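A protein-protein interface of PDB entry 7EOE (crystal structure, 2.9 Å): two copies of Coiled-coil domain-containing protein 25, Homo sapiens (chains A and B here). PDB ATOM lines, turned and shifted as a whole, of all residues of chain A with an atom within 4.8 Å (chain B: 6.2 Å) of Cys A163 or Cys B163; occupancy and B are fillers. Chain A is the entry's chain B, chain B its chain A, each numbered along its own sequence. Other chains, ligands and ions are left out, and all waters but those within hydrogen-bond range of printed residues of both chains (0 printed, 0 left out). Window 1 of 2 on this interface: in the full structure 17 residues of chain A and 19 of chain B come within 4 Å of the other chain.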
ATOM      1  N   ALA A 159      -2.579  -3.011  -1.769  1.00  0.00           N
ATOM      2  CA  ALA A 159      -2.427  -2.399  -0.456  1.00  0.00           C
ATOM      3  C   ALA A 159      -1.257  -3.008   0.307  1.00  0.00           C
ATOM      4  O   ALA A 159      -0.508  -2.289   0.975  1.00  0.00           O
ATOM      5  CB  ALA A 159      -3.728  -2.537   0.333  1.00  0.00           C
ATOM      6  N   GLU A 160      -1.080  -4.330   0.217  1.00  0.00           N
ATOM      7  CA  GLU A 160       0.032  -4.969   0.915  1.00  0.00           C
ATOM      8  C   GLU A 160       1.372  -4.532   0.334  1.00  0.00           C
ATOM      9  O   GLU A 160       2.316  -4.235   1.081  1.00  0.00           O
ATOM     10  CB  GLU A 160      -0.105  -6.490   0.853  1.00  0.00           C
ATOM     11  CG  GLU A 160      -1.466  -7.019   1.263  1.00  0.00           C
ATOM     12  CD  GLU A 160      -1.458  -8.516   1.509  1.00  0.00           C
ATOM     13  OE1 GLU A 160      -2.247  -8.983   2.356  1.00  0.00           O
ATOM     14  OE2 GLU A 160      -0.659  -9.224   0.859  1.00  0.00           O
ATOM     15  N   LYS A 161       1.469  -4.464  -0.997  1.00  0.00           N
ATOM     16  CA  LYS A 161       2.709  -4.008  -1.609  1.00  0.00           C
ATOM     17  C   LYS A 161       3.022  -2.563  -1.257  1.00  0.00           C
ATOM     18  O   LYS A 161       4.196  -2.213  -1.091  1.00  0.00           O
ATOM     19  CB  LYS A 161       2.653  -4.165  -3.129  1.00  0.00           C
ATOM     20  CG  LYS A 161       3.919  -3.657  -3.800  1.00  0.00           C
ATOM     21  CD  LYS A 161       3.997  -3.966  -5.275  1.00  0.00           C
ATOM     22  CE  LYS A 161       5.307  -3.438  -5.829  1.00  0.00           C
ATOM     23  NZ  LYS A 161       5.867  -4.340  -6.858  1.00  0.00           N
ATOM     24  N   GLU A 162       2.004  -1.713  -1.099  1.00  0.00           N
ATOM     25  CA  GLU A 162       2.311  -0.347  -0.694  1.00  0.00           C
ATOM     26  C   GLU A 162       2.498  -0.229   0.818  1.00  0.00           C
ATOM     27  O   GLU A 162       2.956   0.817   1.295  1.00  0.00           O
ATOM     28  CB  GLU A 162       1.237   0.625  -1.189  1.00  0.00           C
ATOM     29  CG  GLU A 162       1.839   1.973  -1.594  1.00  0.00           C
ATOM     30  CD  GLU A 162       1.568   3.117  -0.626  1.00  0.00           C
ATOM     31  OE1 GLU A 162       2.139   4.214  -0.851  1.00  0.00           O
ATOM     32  OE2 GLU A 162       0.783   2.926   0.328  1.00  0.00           O
ATOM     33  N   CYS A 163       2.139  -1.268   1.582  1.00  0.00           N
ATOM     34  CA  CYS A 163       2.617  -1.352   2.958  1.00  0.00           C
ATOM     35  C   CYS A 163       4.093  -1.712   2.989  1.00  0.00           C
ATOM     36  O   CYS A 163       4.828  -1.252   3.871  1.00  0.00           O
ATOM     37  CB  CYS A 163       1.815  -2.381   3.754  1.00  0.00           C
ATOM     38  SG  CYS A 163       0.085  -1.973   4.032  1.00  0.00           S
ATOM     39  N   ARG A 164       4.544  -2.525   2.029  1.00  0.00           N
ATOM     40  CA  ARG A 164       5.972  -2.791   1.906  1.00  0.00           C
ATOM     41  C   ARG A 164       6.717  -1.532   1.481  1.00  0.00           C
ATOM     42  O   ARG A 164       7.779  -1.211   2.031  1.00  0.00           O
ATOM     43  CB  ARG A 164       6.203  -3.922   0.905  1.00  0.00           C
ATOM     44  CG  ARG A 164       7.656  -4.309   0.715  1.00  0.00           C
ATOM     45  CD  ARG A 164       8.022  -4.363  -0.760  1.00  0.00           C
ATOM     46  NE  ARG A 164       8.520  -3.078  -1.237  1.00  0.00           N
ATOM     47  CZ  ARG A 164       9.800  -2.724  -1.212  1.00  0.00           C
ATOM     48  NH1 ARG A 164      10.710  -3.558  -0.728  1.00  0.00           N
ATOM     49  NH2 ARG A 164      10.172  -1.533  -1.664  1.00  0.00           N
ATOM     50  N   ASP A 165       6.159  -0.797   0.515  1.00  0.00           N
ATOM     51  CA  ASP A 165       6.787   0.433   0.051  1.00  0.00           C
ATOM     52  C   ASP A 165       6.794   1.492   1.145  1.00  0.00           C
ATOM     53  O   ASP A 165       7.786   2.208   1.316  1.00  0.00           O
ATOM     54  CB  ASP A 165       6.057   0.956  -1.185  1.00  0.00           C
ATOM     55  CG  ASP A 165       6.349   0.143  -2.428  1.00  0.00           C
ATOM     56  OD1 ASP A 165       7.327  -0.634  -2.421  1.00  0.00           O
ATOM     57  OD2 ASP A 165       5.598   0.284  -3.416  1.00  0.00           O
ATOM     58  N   ARG A 166       5.693   1.604   1.896  1.00  0.00           N
ATOM     59  CA  ARG A 166       5.655   2.528   3.026  1.00  0.00           C
ATOM     60  C   ARG A 166       6.679   2.146   4.086  1.00  0.00           C
ATOM     61  O   ARG A 166       7.338   3.018   4.665  1.00  0.00           O
ATOM     62  CB  ARG A 166       4.249   2.569   3.624  1.00  0.00           C
ATOM     63  CG  ARG A 166       3.270   3.430   2.844  1.00  0.00           C
ATOM     64  CD  ARG A 166       1.842   3.204   3.310  1.00  0.00           C
ATOM     65  NE  ARG A 166       0.879   3.835   2.412  1.00  0.00           N
ATOM     66  CZ  ARG A 166      -0.311   4.290   2.786  1.00  0.00           C
ATOM     67  NH1 ARG A 166      -0.700   4.177   4.047  1.00  0.00           N
ATOM     68  NH2 ARG A 166      -1.118   4.850   1.894  1.00  0.00           N
ATOM     69  N   GLU A 167       6.816   0.847   4.367  1.00  0.00           N
ATOM     70  CA  GLU A 167       7.826   0.395   5.320  1.00  0.00           C
ATOM     71  C   GLU A 167       9.224   0.799   4.864  1.00  0.00           C
ATOM     72  O   GLU A 167      10.028   1.309   5.655  1.00  0.00           O
ATOM     73  CB  GLU A 167       7.724  -1.121   5.506  1.00  0.00           C
ATOM     74  CG  GLU A 167       8.507  -1.668   6.690  1.00  0.00           C
ATOM     75  CD  GLU A 167       9.956  -1.955   6.350  1.00  0.00           C
ATOM     76  OE1 GLU A 167      10.778  -2.057   7.285  1.00  0.00           O
ATOM     77  OE2 GLU A 167      10.276  -2.075   5.149  1.00  0.00           O
ATOM     78  N   TRP B  47      -3.931  -6.665  15.817  1.00  0.00           N
ATOM     79  CA  TRP B  47      -4.940  -7.452  15.123  1.00  0.00           C
ATOM     80  C   TRP B  47      -5.716  -8.320  16.102  1.00  0.00           C
ATOM     81  O   TRP B  47      -5.238  -8.620  17.200  1.00  0.00           O
ATOM     82  CB  TRP B  47      -4.290  -8.339  14.062  1.00  0.00           C
ATOM     83  CG  TRP B  47      -3.580  -7.618  12.958  1.00  0.00           C
ATOM     84  CD1 TRP B  47      -3.304  -6.284  12.884  1.00  0.00           C
ATOM     85  CD2 TRP B  47      -3.067  -8.201  11.754  1.00  0.00           C
ATOM     86  NE1 TRP B  47      -2.640  -6.003  11.713  1.00  0.00           N
ATOM     87  CE2 TRP B  47      -2.482  -7.164  11.003  1.00  0.00           C
ATOM     88  CE3 TRP B  47      -3.035  -9.504  11.244  1.00  0.00           C
ATOM     89  CZ2 TRP B  47      -1.878  -7.387   9.767  1.00  0.00           C
ATOM     90  CZ3 TRP B  47      -2.436  -9.722  10.019  1.00  0.00           C
ATOM     91  CH2 TRP B  47      -1.867  -8.671   9.294  1.00  0.00           C
ATOM     92  N   ARG B 153      11.485  -3.975  11.404  1.00  0.00           N
ATOM     93  CA  ARG B 153      10.736  -3.286  10.368  1.00  0.00           C
ATOM     94  C   ARG B 153      10.270  -1.940  10.901  1.00  0.00           C
ATOM     95  O   ARG B 153      10.284  -1.688  12.106  1.00  0.00           O
ATOM     96  CB  ARG B 153       9.534  -4.121   9.895  1.00  0.00           C
ATOM     97  CG  ARG B 153       9.904  -5.521   9.423  1.00  0.00           C
ATOM     98  CD  ARG B 153       8.818  -6.143   8.554  1.00  0.00           C
ATOM     99  NE  ARG B 153       7.501  -6.076   9.178  1.00  0.00           N
ATOM    100  CZ  ARG B 153       6.496  -5.334   8.725  1.00  0.00           C
ATOM    101  NH1 ARG B 153       6.655  -4.596   7.634  1.00  0.00           N
ATOM    102  NH2 ARG B 153       5.332  -5.333   9.359  1.00  0.00           N
ATOM    103  N   PHE B 154       9.860  -1.067   9.983  1.00  0.00           N
ATOM    104  CA  PHE B 154       9.282   0.230  10.320  1.00  0.00           C
ATOM    105  C   PHE B 154       7.895   0.289   9.684  1.00  0.00           C
ATOM    106  O   PHE B 154       7.659   1.059   8.747  1.00  0.00           O
ATOM    107  CB  PHE B 154      10.160   1.381   9.833  1.00  0.00           C
ATOM    108  CG  PHE B 154      11.600   1.272  10.257  1.00  0.00           C
ATOM    109  CD1 PHE B 154      12.079   1.994  11.337  1.00  0.00           C
ATOM    110  CD2 PHE B 154      12.476   0.448   9.570  1.00  0.00           C
ATOM    111  CE1 PHE B 154      13.402   1.894  11.721  1.00  0.00           C
ATOM    112  CE2 PHE B 154      13.799   0.345   9.950  1.00  0.00           C
ATOM    113  CZ  PHE B 154      14.262   1.071  11.023  1.00  0.00           C
ATOM    114  N   PRO B 155       6.962  -0.514  10.181  1.00  0.00           N
ATOM    115  CA  PRO B 155       5.697  -0.704   9.468  1.00  0.00           C
ATOM    116  C   PRO B 155       4.701   0.412   9.738  1.00  0.00           C
ATOM    117  O   PRO B 155       4.765   1.126  10.740  1.00  0.00           O
ATOM    118  CB  PRO B 155       5.182  -2.039  10.016  1.00  0.00           C
ATOM    119  CG  PRO B 155       5.794  -2.157  11.376  1.00  0.00           C
ATOM    120  CD  PRO B 155       7.008  -1.271  11.443  1.00  0.00           C
ATOM    121  N   ASP B 156       3.764   0.542   8.804  1.00  0.00           N
ATOM    122  CA  ASP B 156       2.620   1.441   8.935  1.00  0.00           C
ATOM    123  C   ASP B 156       1.447   0.565   9.368  1.00  0.00           C
ATOM    124  O   ASP B 156       0.747  -0.022   8.543  1.00  0.00           O
ATOM    125  CB  ASP B 156       2.359   2.180   7.629  1.00  0.00           C
ATOM    126  CG  ASP B 156       1.090   3.009   7.664  1.00  0.00           C
ATOM    127  OD1 ASP B 156       0.703   3.469   8.759  1.00  0.00           O
ATOM    128  OD2 ASP B 156       0.495   3.227   6.589  1.00  0.00           O
ATOM    129  N   ALA B 158      -1.486   0.937  10.713  1.00  0.00           N
ATOM    130  CA  ALA B 158      -2.847   1.210  10.269  1.00  0.00           C
ATOM    131  C   ALA B 158      -3.103   0.586   8.904  1.00  0.00           C
ATOM    132  O   ALA B 158      -4.121  -0.084   8.691  1.00  0.00           O
ATOM    133  CB  ALA B 158      -3.093   2.718  10.233  1.00  0.00           C
ATOM    134  N   ALA B 159      -2.170   0.783   7.968  1.00  0.00           N
ATOM    135  CA  ALA B 159      -2.334   0.235   6.628  1.00  0.00           C
ATOM    136  C   ALA B 159      -2.291  -1.288   6.638  1.00  0.00           C
ATOM    137  O   ALA B 159      -3.057  -1.934   5.917  1.00  0.00           O
ATOM    138  CB  ALA B 159      -1.265   0.800   5.697  1.00  0.00           C
ATOM    139  N   GLU B 160      -1.397  -1.882   7.434  1.00  0.00           N
ATOM    140  CA  GLU B 160      -1.324  -3.340   7.485  1.00  0.00           C
ATOM    141  C   GLU B 160      -2.586  -3.936   8.099  1.00  0.00           C
ATOM    142  O   GLU B 160      -3.119  -4.933   7.595  1.00  0.00           O
ATOM    143  CB  GLU B 160      -0.082  -3.783   8.261  1.00  0.00           C
ATOM    144  CG  GLU B 160       1.209  -3.124   7.798  1.00  0.00           C
ATOM    145  CD  GLU B 160       2.445  -3.815   8.341  1.00  0.00           C
ATOM    146  OE1 GLU B 160       3.484  -3.807   7.647  1.00  0.00           O
ATOM    147  OE2 GLU B 160       2.375  -4.375   9.455  1.00  0.00           O
ATOM    148  N   LYS B 161      -3.086  -3.332   9.181  1.00  0.00           N
ATOM    149  CA  LYS B 161      -4.335  -3.805   9.768  1.00  0.00           C
ATOM    150  C   LYS B 161      -5.504  -3.613   8.808  1.00  0.00           C
ATOM    151  O   LYS B 161      -6.455  -4.407   8.815  1.00  0.00           O
ATOM    152  CB  LYS B 161      -4.600  -3.100  11.098  1.00  0.00           C
ATOM    153  CG  LYS B 161      -5.885  -3.549  11.763  1.00  0.00           C
ATOM    154  CD  LYS B 161      -6.019  -3.023  13.172  1.00  0.00           C
ATOM    155  CE  LYS B 161      -7.302  -3.534  13.798  1.00  0.00           C
ATOM    156  NZ  LYS B 161      -7.127  -3.836  15.237  1.00  0.00           N
ATOM    157  N   GLU B 162      -5.436  -2.593   7.949  1.00  0.00           N
ATOM    158  CA  GLU B 162      -6.470  -2.409   6.937  1.00  0.00           C
ATOM    159  C   GLU B 162      -6.299  -3.352   5.756  1.00  0.00           C
ATOM    160  O   GLU B 162      -7.278  -3.632   5.053  1.00  0.00           O
ATOM    161  CB  GLU B 162      -6.441  -0.958   6.439  1.00  0.00           C
ATOM    162  CG  GLU B 162      -7.498  -0.590   5.400  1.00  0.00           C
ATOM    163  CD  GLU B 162      -8.849  -0.249   5.984  1.00  0.00           C
ATOM    164  OE1 GLU B 162      -9.854  -0.421   5.262  1.00  0.00           O
ATOM    165  OE2 GLU B 162      -8.907   0.201   7.146  1.00  0.00           O
ATOM    166  N   CYS B 163      -5.106  -3.918   5.581  1.00  0.00           N
ATOM    167  CA  CYS B 163      -4.948  -5.033   4.659  1.00  0.00           C
ATOM    168  C   CYS B 163      -5.516  -6.313   5.247  1.00  0.00           C
ATOM    169  O   CYS B 163      -6.052  -7.148   4.511  1.00  0.00           O
ATOM    170  CB  CYS B 163      -3.473  -5.219   4.311  1.00  0.00           C
ATOM    171  SG  CYS B 163      -2.761  -3.850   3.387  1.00  0.00           S
ATOM    172  N   ARG B 164      -5.417  -6.478   6.566  1.00  0.00           N
ATOM    173  CA  ARG B 164      -6.038  -7.632   7.205  1.00  0.00           C
ATOM    174  C   ARG B 164      -7.559  -7.550   7.129  1.00  0.00           C
ATOM    175  O   ARG B 164      -8.226  -8.535   6.779  1.00  0.00           O
ATOM    176  CB  ARG B 164      -5.564  -7.728   8.655  1.00  0.00           C
ATOM    177  CG  ARG B 164      -6.134  -8.897   9.423  1.00  0.00           C
ATOM    178  CD  ARG B 164      -6.690  -8.441  10.757  1.00  0.00           C
ATOM    179  NE  ARG B 164      -7.683  -9.376  11.271  1.00  0.00           N
ATOM    180  CZ  ARG B 164      -8.984  -9.285  11.018  1.00  0.00           C
ATOM    181  NH1 ARG B 164      -9.446  -8.297  10.265  1.00  0.00           N
ATOM    182  NH2 ARG B 164      -9.823 -10.178  11.523  1.00  0.00           N
ATOM    183  N   ASP B 165      -8.123  -6.374   7.419  1.00  0.00           N
ATOM    184  CA  ASP B 165      -9.573  -6.217   7.350  1.00  0.00           C
ATOM    185  C   ASP B 165     -10.072  -6.331   5.914  1.00  0.00           C
ATOM    186  O   ASP B 165     -11.119  -6.940   5.662  1.00  0.00           O
ATOM    187  CB  ASP B 165      -9.988  -4.882   7.968  1.00  0.00           C
ATOM    188  CG  ASP B 165      -9.920  -4.895   9.484  1.00  0.00           C
ATOM    189  OD1 ASP B 165      -9.920  -3.803  10.087  1.00  0.00           O
ATOM    190  OD2 ASP B 165      -9.847  -5.994  10.071  1.00  0.00           O
ATOM    191  N   ARG B 166      -9.336  -5.758   4.957  1.00  0.00           N
ATOM    192  CA  ARG B 166      -9.711  -5.938   3.559  1.00  0.00           C
ATOM    193  C   ARG B 166      -9.656  -7.408   3.160  1.00  0.00           C
ATOM    194  O   ARG B 166     -10.532  -7.897   2.439  1.00  0.00           O
ATOM    195  CB  ARG B 166      -8.807  -5.107   2.652  1.00  0.00           C
ATOM    196  CG  ARG B 166      -9.168  -3.636   2.588  1.00  0.00           C
ATOM    197  CD  ARG B 166      -8.080  -2.863   1.876  1.00  0.00           C
ATOM    198  NE  ARG B 166      -8.256  -1.421   2.004  1.00  0.00           N
ATOM    199  CZ  ARG B 166      -7.868  -0.542   1.088  1.00  0.00           C
ATOM    200  NH1 ARG B 166      -7.282  -0.960  -0.026  1.00  0.00           N
ATOM    201  NH2 ARG B 166      -8.063   0.754   1.286  1.00  0.00           N
ATOM    202  N   GLU B 167      -8.630  -8.129   3.622  1.00  0.00           N
ATOM    203  CA  GLU B 167      -8.517  -9.555   3.327  1.00  0.00           C
ATOM    204  C   GLU B 167      -9.725 -10.329   3.846  1.00  0.00           C
ATOM    205  O   GLU B 167     -10.303 -11.157   3.126  1.00  0.00           O
ATOM    206  CB  GLU B 167      -7.215 -10.100   3.923  1.00  0.00           C
ATOM    207  CG  GLU B 167      -6.822 -11.487   3.444  1.00  0.00           C
ATOM    208  CD  GLU B 167      -7.473 -12.589   4.254  1.00  0.00           C
ATOM    209  OE1 GLU B 167      -7.538 -13.734   3.760  1.00  0.00           O
ATOM    210  OE2 GLU B 167      -7.927 -12.310   5.383  1.00  0.00           O
ATOM    211  N   GLU B 168     -10.127 -10.068   5.095  1.00  0.00           N
ATOM    212  CA  GLU B 168     -11.287 -10.763   5.649  1.00  0.00           C
ATOM    213  C   GLU B 168     -12.559 -10.404   4.884  1.00  0.00           C
ATOM    214  O   GLU B 168     -13.421 -11.263   4.653  1.00  0.00           O
ATOM    215  CB  GLU B 168     -11.428 -10.471   7.149  1.00  0.00           C
ATOM    216  CG  GLU B 168     -12.117  -9.166   7.529  1.00  0.00           C
ATOM    217  CD  GLU B 168     -12.775  -9.226   8.899  1.00  0.00           C
ATOM    218  OE1 GLU B 168     -12.994  -8.155   9.506  1.00  0.00           O
ATOM    219  OE2 GLU B 168     -13.075 -10.348   9.364  1.00  0.00           O
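The backbone NH of Phe B154 sits at hydrogen-bond distance from the side-chain carboxylate of Glu A167 (3.0 Å). The backbone NH of Glu B160 is in hydrogen-bond range of the side-chain sulfur of Cys A163 (3.7 Å). O of Ala B159 lies close to SG of Cys A163, 3.7 Å away. The guanidinium group (NH1) of Arg A166 lies within salt-bridge range of the side-chain carboxylate (OD2) of Asp B156 (3.0 Å). The side-chain sulfur (SG) of Cys A163 sits at hydrogen-bond distance from the side-chain sulfur (SG) of Cys B163, 3.5 Å away. SG of Cys B163 sits close to O of Ala A159, at 3.7 Å. The side-chain sulfur (SG) of Cys B163 lies within hydrogen-bond range of the backbone NH (N) of Glu A160, at 3.6 Å.
NE of Arg B166 lies within salt-bridge range of OE1 of Glu B162. The side-chain carboxylate (OE2) of Glu A162 lies within salt-bridge range of the guanidinium group (NH2) of Arg A166, at 3.1 Å. OE1 of Glu B160 is in salt-bridge range of NH2 of Arg B153, 2.9 Å away. The backbone carbonyl oxygen (O) of Ala B159 lies within hydrogen-bond range of the side-chain sulfur (SG) of Cys B163 (3.2 Å). SG of Cys A163 sits at hydrogen-bond distance from O of Ala A159.
Among the printed residues, merely in contact across the chains: Glu A167 with Arg B153, Arg A166 with Ala B159, Ala A159 with Arg B166 and Glu A167 with Pro B155.
Cys A163 touches just these residues of chain B: Ala B159, Glu B160 and Cys B163. Printed residues of chain B within 4 Å of Glu A167: Arg B153, Phe B154 and Pro B155. Trp B47 touches none of the printed residues of chain A. Printed residues of chain A within 4 Å of Pro B155: Glu A167 (3.99 Å). Of chain A, only Ala A159 (3.5 Å), Glu A160 (3.6 Å) and Cys A163 (3.5 Å) come within 4 Å of Cys B163. The nearest residue of chain B that does not touch Cys A163 is Asp B156 (5.0 Å). The nearest printed residue of chain A that does not touch Cys B163 is Lys A161 (6.1 Å). The nearest printed residue of chain B that does not touch Glu A167 is Asp B156 (5.4 Å).
Of the 9 printed residues of chain A, 5 touch a printed residue of chain B. Hydrophobic or aromatic side chains of chain A that line the printed part of chain B: Ala A159. Hydrophobic or aromatic side chains of chain B within 4 Å of the printed part of chain A: Phe B154 and Ala B159.
Ala A159 touches Cys B163, and with the chains exchanged Cys A163 touches Ala B159. Ala A159 touches Arg B166, and with the chains exchanged Arg A166 touches Ala B159. Glu A160 touches Cys B163, and with the chains exchanged Cys A163 touches Glu B160. Cys A163 touches its own counterpart, Cys B163. Of the 11 pairs that touch across the chains among the printed residues, 7 have their exchanged pair printed and touching as well.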
